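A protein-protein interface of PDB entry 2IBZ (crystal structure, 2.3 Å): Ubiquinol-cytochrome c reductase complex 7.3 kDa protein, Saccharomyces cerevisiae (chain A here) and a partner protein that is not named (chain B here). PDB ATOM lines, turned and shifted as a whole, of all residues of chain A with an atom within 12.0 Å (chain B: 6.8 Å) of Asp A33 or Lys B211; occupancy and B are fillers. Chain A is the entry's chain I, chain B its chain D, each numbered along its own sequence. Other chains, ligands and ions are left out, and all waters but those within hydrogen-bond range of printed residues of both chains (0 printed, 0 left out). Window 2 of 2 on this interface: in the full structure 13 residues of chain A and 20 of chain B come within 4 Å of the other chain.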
ATOM      1  N   GLY A  24      13.362  -1.638  20.356  1.00  0.00           N
ATOM      2  CA  GLY A  24      12.154  -2.233  20.889  1.00  0.00           C
ATOM      3  C   GLY A  24      10.910  -1.620  20.267  1.00  0.00           C
ATOM      4  O   GLY A  24       9.913  -2.317  20.067  1.00  0.00           O
ATOM      5  N   ALA A  25      10.975  -0.326  19.947  1.00  0.00           N
ATOM      6  CA  ALA A  25       9.852   0.402  19.342  1.00  0.00           C
ATOM      7  C   ALA A  25       9.498  -0.117  17.947  1.00  0.00           C
ATOM      8  O   ALA A  25       8.320  -0.227  17.611  1.00  0.00           O
ATOM      9  CB  ALA A  25      10.149   1.913  19.293  1.00  0.00           C
ATOM     10  N   PHE A  26      10.514  -0.418  17.138  1.00  0.00           N
ATOM     11  CA  PHE A  26      10.297  -0.949  15.786  1.00  0.00           C
ATOM     12  C   PHE A  26       9.603  -2.311  15.870  1.00  0.00           C
ATOM     13  O   PHE A  26       8.724  -2.622  15.061  1.00  0.00           O
ATOM     14  CB  PHE A  26      11.625  -1.111  15.029  1.00  0.00           C
ATOM     15  CG  PHE A  26      12.199   0.179  14.484  1.00  0.00           C
ATOM     16  CD1 PHE A  26      12.616   0.256  13.149  1.00  0.00           C
ATOM     17  CD2 PHE A  26      12.383   1.294  15.307  1.00  0.00           C
ATOM     18  CE1 PHE A  26      13.215   1.429  12.639  1.00  0.00           C
ATOM     19  CE2 PHE A  26      12.978   2.466  14.814  1.00  0.00           C
ATOM     20  CZ  PHE A  26      13.396   2.536  13.481  1.00  0.00           C
ATOM     21  N   VAL A  27      10.006  -3.113  16.855  1.00  0.00           N
ATOM     22  CA  VAL A  27       9.442  -4.443  17.075  1.00  0.00           C
ATOM     23  C   VAL A  27       7.986  -4.303  17.487  1.00  0.00           C
ATOM     24  O   VAL A  27       7.097  -4.938  16.905  1.00  0.00           O
ATOM     25  CB  VAL A  27      10.188  -5.201  18.206  1.00  0.00           C
ATOM     26  CG1 VAL A  27       9.582  -6.589  18.412  1.00  0.00           C
ATOM     27  CG2 VAL A  27      11.670  -5.304  17.894  1.00  0.00           C
ATOM     28  N   PHE A  28       7.764  -3.463  18.499  1.00  0.00           N
ATOM     29  CA  PHE A  28       6.433  -3.201  19.036  1.00  0.00           C
ATOM     30  C   PHE A  28       5.456  -2.808  17.938  1.00  0.00           C
ATOM     31  O   PHE A  28       4.375  -3.384  17.818  1.00  0.00           O
ATOM     32  CB  PHE A  28       6.494  -2.083  20.087  1.00  0.00           C
ATOM     33  CG  PHE A  28       5.148  -1.704  20.647  1.00  0.00           C
ATOM     34  CD1 PHE A  28       4.629  -2.369  21.753  1.00  0.00           C
ATOM     35  CD2 PHE A  28       4.386  -0.702  20.048  1.00  0.00           C
ATOM     36  CE1 PHE A  28       3.370  -2.045  22.254  1.00  0.00           C
ATOM     37  CE2 PHE A  28       3.124  -0.370  20.542  1.00  0.00           C
ATOM     38  CZ  PHE A  28       2.617  -1.042  21.646  1.00  0.00           C
ATOM     39  N   GLN A  29       5.856  -1.831  17.132  1.00  0.00           N
ATOM     40  CA  GLN A  29       5.022  -1.338  16.052  1.00  0.00           C
ATOM     41  C   GLN A  29       4.408  -2.449  15.205  1.00  0.00           C
ATOM     42  O   GLN A  29       3.201  -2.459  14.971  1.00  0.00           O
ATOM     43  CB  GLN A  29       5.824  -0.377  15.182  1.00  0.00           C
ATOM     44  CG  GLN A  29       4.981   0.393  14.189  1.00  0.00           C
ATOM     45  CD  GLN A  29       5.638   1.689  13.750  1.00  0.00           C
ATOM     46  OE1 GLN A  29       5.472   2.732  14.397  1.00  0.00           O
ATOM     47  NE2 GLN A  29       6.384   1.634  12.647  1.00  0.00           N
ATOM     48  N   THR A  30       5.230  -3.415  14.804  1.00  0.00           N
ATOM     49  CA  THR A  30       4.772  -4.529  13.983  1.00  0.00           C
ATOM     50  C   THR A  30       3.882  -5.510  14.745  1.00  0.00           C
ATOM     51  O   THR A  30       2.802  -5.866  14.275  1.00  0.00           O
ATOM     52  CB  THR A  30       5.970  -5.296  13.374  1.00  0.00           C
ATOM     53  OG1 THR A  30       6.762  -4.393  12.591  1.00  0.00           O
ATOM     54  CG2 THR A  30       5.483  -6.440  12.479  1.00  0.00           C
ATOM     55  N   VAL A  31       4.358  -5.955  15.904  1.00  0.00           N
ATOM     56  CA  VAL A  31       3.633  -6.902  16.743  1.00  0.00           C
ATOM     57  C   VAL A  31       2.262  -6.359  17.133  1.00  0.00           C
ATOM     58  O   VAL A  31       1.233  -7.003  16.914  1.00  0.00           O
ATOM     59  CB  VAL A  31       4.433  -7.219  18.041  1.00  0.00           C
ATOM     60  CG1 VAL A  31       3.631  -8.144  18.957  1.00  0.00           C
ATOM     61  CG2 VAL A  31       5.769  -7.850  17.694  1.00  0.00           C
ATOM     62  N   PHE A  32       2.266  -5.161  17.705  1.00  0.00           N
ATOM     63  CA  PHE A  32       1.050  -4.493  18.156  1.00  0.00           C
ATOM     64  C   PHE A  32       0.000  -4.338  17.053  1.00  0.00           C
ATOM     65  O   PHE A  32      -1.180  -4.586  17.281  1.00  0.00           O
ATOM     66  CB  PHE A  32       1.410  -3.128  18.738  1.00  0.00           C
ATOM     67  CG  PHE A  32       0.273  -2.451  19.430  1.00  0.00           C
ATOM     68  CD1 PHE A  32      -0.315  -3.030  20.549  1.00  0.00           C
ATOM     69  CD2 PHE A  32      -0.207  -1.226  18.969  1.00  0.00           C
ATOM     70  CE1 PHE A  32      -1.360  -2.402  21.200  1.00  0.00           C
ATOM     71  CE2 PHE A  32      -1.249  -0.592  19.611  1.00  0.00           C
ATOM     72  CZ  PHE A  32      -1.828  -1.178  20.728  1.00  0.00           C
ATOM     73  N   ASP A  33       0.442  -3.950  15.860  1.00  0.00           N
ATOM     74  CA  ASP A  33      -0.460  -3.761  14.732  1.00  0.00           C
ATOM     75  C   ASP A  33      -1.172  -5.049  14.333  1.00  0.00           C
ATOM     76  O   ASP A  33      -2.375  -5.040  14.084  1.00  0.00           O
ATOM     77  CB  ASP A  33       0.300  -3.199  13.530  1.00  0.00           C
ATOM     78  CG  ASP A  33      -0.624  -2.727  12.427  1.00  0.00           C
ATOM     79  OD1 ASP A  33      -1.551  -1.959  12.730  1.00  0.00           O
ATOM     80  OD2 ASP A  33      -0.425  -3.115  11.254  1.00  0.00           O
ATOM     81  N   THR A  34      -0.431  -6.155  14.287  1.00  0.00           N
ATOM     82  CA  THR A  34      -1.002  -7.449  13.915  1.00  0.00           C
ATOM     83  C   THR A  34      -1.998  -7.902  14.977  1.00  0.00           C
ATOM     84  O   THR A  34      -3.112  -8.314  14.657  1.00  0.00           O
ATOM     85  CB  THR A  34       0.100  -8.528  13.710  1.00  0.00           C
ATOM     86  OG1 THR A  34       0.995  -8.111  12.668  1.00  0.00           O
ATOM     87  CG2 THR A  34      -0.523  -9.869  13.313  1.00  0.00           C
ATOM     88  N   ALA A  35      -1.610  -7.775  16.241  1.00  0.00           N
ATOM     89  CA  ALA A  35      -2.481  -8.156  17.347  1.00  0.00           C
ATOM     90  C   ALA A  35      -3.830  -7.419  17.301  1.00  0.00           C
ATOM     91  O   ALA A  35      -4.881  -8.035  17.504  1.00  0.00           O
ATOM     92  CB  ALA A  35      -1.782  -7.900  18.681  1.00  0.00           C
ATOM     93  N   ILE A  36      -3.792  -6.112  17.016  1.00  0.00           N
ATOM     94  CA  ILE A  36      -4.990  -5.278  16.946  1.00  0.00           C
ATOM     95  C   ILE A  36      -5.812  -5.586  15.702  1.00  0.00           C
ATOM     96  O   ILE A  36      -7.031  -5.726  15.789  1.00  0.00           O
ATOM     97  CB  ILE A  36      -4.636  -3.753  16.971  1.00  0.00           C
ATOM     98  CG1 ILE A  36      -3.936  -3.393  18.281  1.00  0.00           C
ATOM     99  CG2 ILE A  36      -5.894  -2.891  16.806  1.00  0.00           C
ATOM    100  CD1 ILE A  36      -4.744  -3.718  19.508  1.00  0.00           C
ATOM    101  N   THR A  37      -5.163  -5.668  14.546  1.00  0.00           N
ATOM    102  CA  THR A  37      -5.891  -5.981  13.317  1.00  0.00           C
ATOM    103  C   THR A  37      -6.599  -7.333  13.453  1.00  0.00           C
ATOM    104  O   THR A  37      -7.748  -7.490  13.024  1.00  0.00           O
ATOM    105  CB  THR A  37      -4.960  -6.052  12.097  1.00  0.00           C
ATOM    106  OG1 THR A  37      -4.360  -4.770  11.867  1.00  0.00           O
ATOM    107  CG2 THR A  37      -5.747  -6.479  10.859  1.00  0.00           C
ATOM    108  N   SER A  38      -5.914  -8.301  14.065  1.00  0.00           N
ATOM    109  CA  SER A  38      -6.484  -9.633  14.258  1.00  0.00           C
ATOM    110  C   SER A  38      -7.745  -9.575  15.095  1.00  0.00           C
ATOM    111  O   SER A  38      -8.800 -10.050  14.670  1.00  0.00           O
ATOM    112  CB  SER A  38      -5.477 -10.586  14.911  1.00  0.00           C
ATOM    113  OG  SER A  38      -4.475 -10.952  13.983  1.00  0.00           O
ATOM    114  N   TRP A  39      -7.631  -8.988  16.281  1.00  0.00           N
ATOM    115  CA  TRP A  39      -8.771  -8.863  17.176  1.00  0.00           C
ATOM    116  C   TRP A  39      -9.919  -8.128  16.480  1.00  0.00           C
ATOM    117  O   TRP A  39     -11.050  -8.604  16.466  1.00  0.00           O
ATOM    118  CB  TRP A  39      -8.360  -8.121  18.449  1.00  0.00           C
ATOM    119  CG  TRP A  39      -9.456  -8.029  19.454  1.00  0.00           C
ATOM    120  CD1 TRP A  39      -9.721  -8.916  20.453  1.00  0.00           C
ATOM    121  CD2 TRP A  39     -10.474  -7.021  19.527  1.00  0.00           C
ATOM    122  NE1 TRP A  39     -10.849  -8.535  21.140  1.00  0.00           N
ATOM    123  CE2 TRP A  39     -11.333  -7.375  20.594  1.00  0.00           C
ATOM    124  CE3 TRP A  39     -10.748  -5.856  18.794  1.00  0.00           C
ATOM    125  CZ2 TRP A  39     -12.450  -6.608  20.948  1.00  0.00           C
ATOM    126  CZ3 TRP A  39     -11.854  -5.094  19.140  1.00  0.00           C
ATOM    127  CH2 TRP A  39     -12.694  -5.473  20.210  1.00  0.00           C
ATOM    128  N   TYR A  40      -9.603  -7.000  15.850  1.00  0.00           N
ATOM    129  CA  TYR A  40     -10.597  -6.181  15.163  1.00  0.00           C
ATOM    130  C   TYR A  40     -11.357  -6.947  14.082  1.00  0.00           C
ATOM    131  O   TYR A  40     -12.589  -6.920  14.054  1.00  0.00           O
ATOM    132  CB  TYR A  40      -9.922  -4.936  14.568  1.00  0.00           C
ATOM    133  CG  TYR A  40     -10.860  -3.849  14.095  1.00  0.00           C
ATOM    134  CD1 TYR A  40     -11.578  -3.065  15.010  1.00  0.00           C
ATOM    135  CD2 TYR A  40     -10.987  -3.559  12.735  1.00  0.00           C
ATOM    136  CE1 TYR A  40     -12.392  -2.018  14.579  1.00  0.00           C
ATOM    137  CE2 TYR A  40     -11.796  -2.515  12.293  1.00  0.00           C
ATOM    138  CZ  TYR A  40     -12.495  -1.753  13.218  1.00  0.00           C
ATOM    139  OH  TYR A  40     -13.298  -0.738  12.770  1.00  0.00           O
ATOM    140  N   GLU A  41     -10.627  -7.614  13.189  1.00  0.00           N
ATOM    141  CA  GLU A  41     -11.262  -8.376  12.112  1.00  0.00           C
ATOM    142  C   GLU A  41     -12.096  -9.556  12.628  1.00  0.00           C
ATOM    143  O   GLU A  41     -13.138  -9.884  12.061  1.00  0.00           O
ATOM    144  CB  GLU A  41     -10.225  -8.863  11.102  1.00  0.00           C
ATOM    145  CG  GLU A  41      -9.619  -7.759  10.278  1.00  0.00           C
ATOM    146  CD  GLU A  41      -8.865  -8.276   9.069  1.00  0.00           C
ATOM    147  OE1 GLU A  41      -8.828  -7.546   8.053  1.00  0.00           O
ATOM    148  OE2 GLU A  41      -8.307  -9.400   9.129  1.00  0.00           O
ATOM    149  N   ASN A  42     -11.628 -10.182  13.706  1.00  0.00           N
ATOM    150  CA  ASN A  42     -12.335 -11.298  14.317  1.00  0.00           C
ATOM    151  C   ASN A  42     -13.618 -10.789  14.978  1.00  0.00           C
ATOM    152  O   ASN A  42     -14.693 -11.364  14.792  1.00  0.00           O
ATOM    153  CB  ASN A  42     -11.443 -11.990  15.356  1.00  0.00           C
ATOM    154  CG  ASN A  42     -12.139 -13.160  16.030  1.00  0.00           C
ATOM    155  OD1 ASN A  42     -12.335 -14.215  15.419  1.00  0.00           O
ATOM    156  ND2 ASN A  42     -12.541 -12.971  17.286  1.00  0.00           N
ATOM    157  N   LYS B 206     -11.755   3.691  12.917  1.00  0.00           N
ATOM    158  CA  LYS B 206     -11.966   3.102  14.237  1.00  0.00           C
ATOM    159  C   LYS B 206     -10.872   2.123  14.652  1.00  0.00           C
ATOM    160  O   LYS B 206     -10.627   1.916  15.839  1.00  0.00           O
ATOM    161  CB  LYS B 206     -13.308   2.393  14.298  1.00  0.00           C
ATOM    162  CG  LYS B 206     -14.521   3.290  14.147  1.00  0.00           C
ATOM    163  CD  LYS B 206     -15.694   2.624  14.818  1.00  0.00           C
ATOM    164  CE  LYS B 206     -16.986   3.208  14.356  1.00  0.00           C
ATOM    165  NZ  LYS B 206     -18.112   2.469  14.970  1.00  0.00           N
ATOM    166  N   ARG B 207     -10.258   1.479  13.667  1.00  0.00           N
ATOM    167  CA  ARG B 207      -9.185   0.530  13.924  1.00  0.00           C
ATOM    168  C   ARG B 207      -7.967   1.325  14.428  1.00  0.00           C
ATOM    169  O   ARG B 207      -7.307   0.929  15.394  1.00  0.00           O
ATOM    170  CB  ARG B 207      -8.855  -0.214  12.629  1.00  0.00           C
ATOM    171  CG  ARG B 207      -8.027  -1.460  12.808  1.00  0.00           C
ATOM    172  CD  ARG B 207      -7.331  -1.822  11.503  1.00  0.00           C
ATOM    173  NE  ARG B 207      -5.901  -1.803  11.740  1.00  0.00           N
ATOM    174  CZ  ARG B 207      -5.026  -1.088  11.049  1.00  0.00           C
ATOM    175  NH1 ARG B 207      -3.746  -1.136  11.382  1.00  0.00           N
ATOM    176  NH2 ARG B 207      -5.412  -0.371  10.006  1.00  0.00           N
ATOM    177  N   LEU B 208      -7.687   2.454  13.771  1.00  0.00           N
ATOM    178  CA  LEU B 208      -6.581   3.327  14.163  1.00  0.00           C
ATOM    179  C   LEU B 208      -6.850   3.947  15.529  1.00  0.00           C
ATOM    180  O   LEU B 208      -5.941   4.082  16.353  1.00  0.00           O
ATOM    181  CB  LEU B 208      -6.362   4.435  13.142  1.00  0.00           C
ATOM    182  CG  LEU B 208      -5.827   4.016  11.780  1.00  0.00           C
ATOM    183  CD1 LEU B 208      -5.442   5.263  10.997  1.00  0.00           C
ATOM    184  CD2 LEU B 208      -4.613   3.118  11.956  1.00  0.00           C
ATOM    185  N   GLY B 209      -8.110   4.288  15.777  1.00  0.00           N
ATOM    186  CA  GLY B 209      -8.463   4.871  17.055  1.00  0.00           C
ATOM    187  C   GLY B 209      -8.149   3.926  18.190  1.00  0.00           C
ATOM    188  O   GLY B 209      -7.664   4.350  19.237  1.00  0.00           O
ATOM    189  N   LEU B 210      -8.436   2.641  17.980  1.00  0.00           N
ATOM    190  CA  LEU B 210      -8.188   1.603  18.972  1.00  0.00           C
ATOM    191  C   LEU B 210      -6.710   1.552  19.370  1.00  0.00           C
ATOM    192  O   LEU B 210      -6.384   1.524  20.558  1.00  0.00           O
ATOM    193  CB  LEU B 210      -8.665   0.250  18.435  1.00  0.00           C
ATOM    194  CG  LEU B 210      -8.506  -0.986  19.333  1.00  0.00           C
ATOM    195  CD1 LEU B 210      -9.105  -0.754  20.722  1.00  0.00           C
ATOM    196  CD2 LEU B 210      -9.170  -2.175  18.646  1.00  0.00           C
ATOM    197  N   LYS B 211      -5.820   1.598  18.383  1.00  0.00           N
ATOM    198  CA  LYS B 211      -4.381   1.582  18.657  1.00  0.00           C
ATOM    199  C   LYS B 211      -3.957   2.878  19.338  1.00  0.00           C
ATOM    200  O   LYS B 211      -3.187   2.854  20.309  1.00  0.00           O
ATOM    201  CB  LYS B 211      -3.564   1.443  17.368  1.00  0.00           C
ATOM    202  CG  LYS B 211      -3.846   0.193  16.534  1.00  0.00           C
ATOM    203  CD  LYS B 211      -3.192   0.283  15.149  1.00  0.00           C
ATOM    204  CE  LYS B 211      -1.667   0.276  15.227  1.00  0.00           C
ATOM    205  NZ  LYS B 211      -1.055   0.736  13.944  1.00  0.00           N
ATOM    206  N   THR B 212      -4.444   4.007  18.811  1.00  0.00           N
ATOM    207  CA  THR B 212      -4.109   5.325  19.348  1.00  0.00           C
ATOM    208  C   THR B 212      -4.528   5.468  20.812  1.00  0.00           C
ATOM    209  O   THR B 212      -3.743   5.918  21.659  1.00  0.00           O
ATOM    210  CB  THR B 212      -4.753   6.457  18.515  1.00  0.00           C
ATOM    211  OG1 THR B 212      -4.295   6.377  17.155  1.00  0.00           O
ATOM    212  CG2 THR B 212      -4.360   7.812  19.087  1.00  0.00           C
ATOM    213  N   VAL B 213      -5.749   5.052  21.117  1.00  0.00           N
ATOM    214  CA  VAL B 213      -6.244   5.142  22.479  1.00  0.00           C
ATOM    215  C   VAL B 213      -5.517   4.212  23.443  1.00  0.00           C
ATOM    216  O   VAL B 213      -5.330   4.556  24.604  1.00  0.00           O
ATOM    217  CB  VAL B 213      -7.762   4.925  22.528  1.00  0.00           C
ATOM    218  CG1 VAL B 213      -8.232   4.715  23.958  1.00  0.00           C
ATOM    219  CG2 VAL B 213      -8.470   6.143  21.900  1.00  0.00           C
ATOM    220  N   ILE B 214      -5.093   3.039  22.975  1.00  0.00           N
ATOM    221  CA  ILE B 214      -4.376   2.126  23.856  1.00  0.00           C
ATOM    222  C   ILE B 214      -3.003   2.687  24.203  1.00  0.00           C
ATOM    223  O   ILE B 214      -2.617   2.720  25.374  1.00  0.00           O
ATOM    224  CB  ILE B 214      -4.260   0.703  23.250  1.00  0.00           C
ATOM    225  CG1 ILE B 214      -5.624   0.008  23.332  1.00  0.00           C
ATOM    226  CG2 ILE B 214      -3.206  -0.132  23.991  1.00  0.00           C
ATOM    227  CD1 ILE B 214      -5.668  -1.339  22.636  1.00  0.00           C
ATOM    228  N   ILE B 215      -2.281   3.164  23.198  1.00  0.00           N
ATOM    229  CA  ILE B 215      -0.954   3.733  23.430  1.00  0.00           C
ATOM    230  C   ILE B 215      -1.025   4.973  24.326  1.00  0.00           C
ATOM    231  O   ILE B 215      -0.292   5.072  25.327  1.00  0.00           O
ATOM    232  CB  ILE B 215      -0.266   4.098  22.097  1.00  0.00           C
ATOM    233  CG1 ILE B 215       0.058   2.828  21.314  1.00  0.00           C
ATOM    234  CG2 ILE B 215       1.006   4.915  22.348  1.00  0.00           C
ATOM    235  CD1 ILE B 215       0.341   3.083  19.866  1.00  0.00           C
ATOM    236  N   LEU B 216      -1.940   5.891  24.007  1.00  0.00           N
ATOM    237  CA  LEU B 216      -2.064   7.111  24.799  1.00  0.00           C
ATOM    238  C   LEU B 216      -2.487   6.839  26.236  1.00  0.00           C
ATOM    239  O   LEU B 216      -1.980   7.481  27.151  1.00  0.00           O
ATOM    240  CB  LEU B 216      -2.974   8.151  24.110  1.00  0.00           C
ATOM    241  CG  LEU B 216      -2.331   8.821  22.893  1.00  0.00           C
ATOM    242  CD1 LEU B 216      -3.361   9.567  22.044  1.00  0.00           C
ATOM    243  CD2 LEU B 216      -1.224   9.741  23.350  1.00  0.00           C
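The guanidinium group (NH1) of Arg B207 is in salt-bridge range of the side-chain carboxylate (OD1) of Asp A33, 2.7 Å away. NE of Arg B207 is in hydrogen-bond range of OG1 of Thr A37, at 3.3 Å. The side-chain carboxylate (OD1) of Asp A33 lies within salt-bridge range of the side-chain amino group (NZ) of Lys B211, at 3.0 Å.
The backbone carbonyl oxygen of Asp A33 is in hydrogen-bond range of the side-chain hydroxyl of Thr A37, 3.0 Å away.
Among the printed residues, merely in contact across the chains: Tyr A40 with Lys B206, Tyr A40 with Arg B207, Phe A32 with Ile B214, Ile A36 with Lys B211, Phe A32 with Lys B211, Ile A36 with Leu B210 and Trp A39 with Leu B210.
Asp A33 touches just these residues of chain B: Arg B207 (2.7 Å) and Lys B211 (3.0 Å). Of chain A, only Phe A32, Asp A33 and Ile A36 come within 4 Å of Lys B211. Of chain A, only Asp A33, Thr A37 and Tyr A40 come within 4 Å of Arg B207. No residue of chain A comes within 4 Å of Leu B208. No residue of chain A comes within 4 Å of Gly B209. No residue of chain A comes within 4 Å of Val B213. Ile B214 touches just one residue of chain A: Phe A32. Printed residues of chain A within 4 Å of Leu B210: Ile A36 (3.8 Å) and Trp A39 (3.996 Å). Of the printed residues of chain B, Phe A32 touches Lys B211 and Ile B214. Ala A35 touches none of the printed residues of chain B.
Of the 11 printed residues of chain B, 5 touch a printed residue of chain A. Among the printed residues, 10 pairs touch across the chains.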
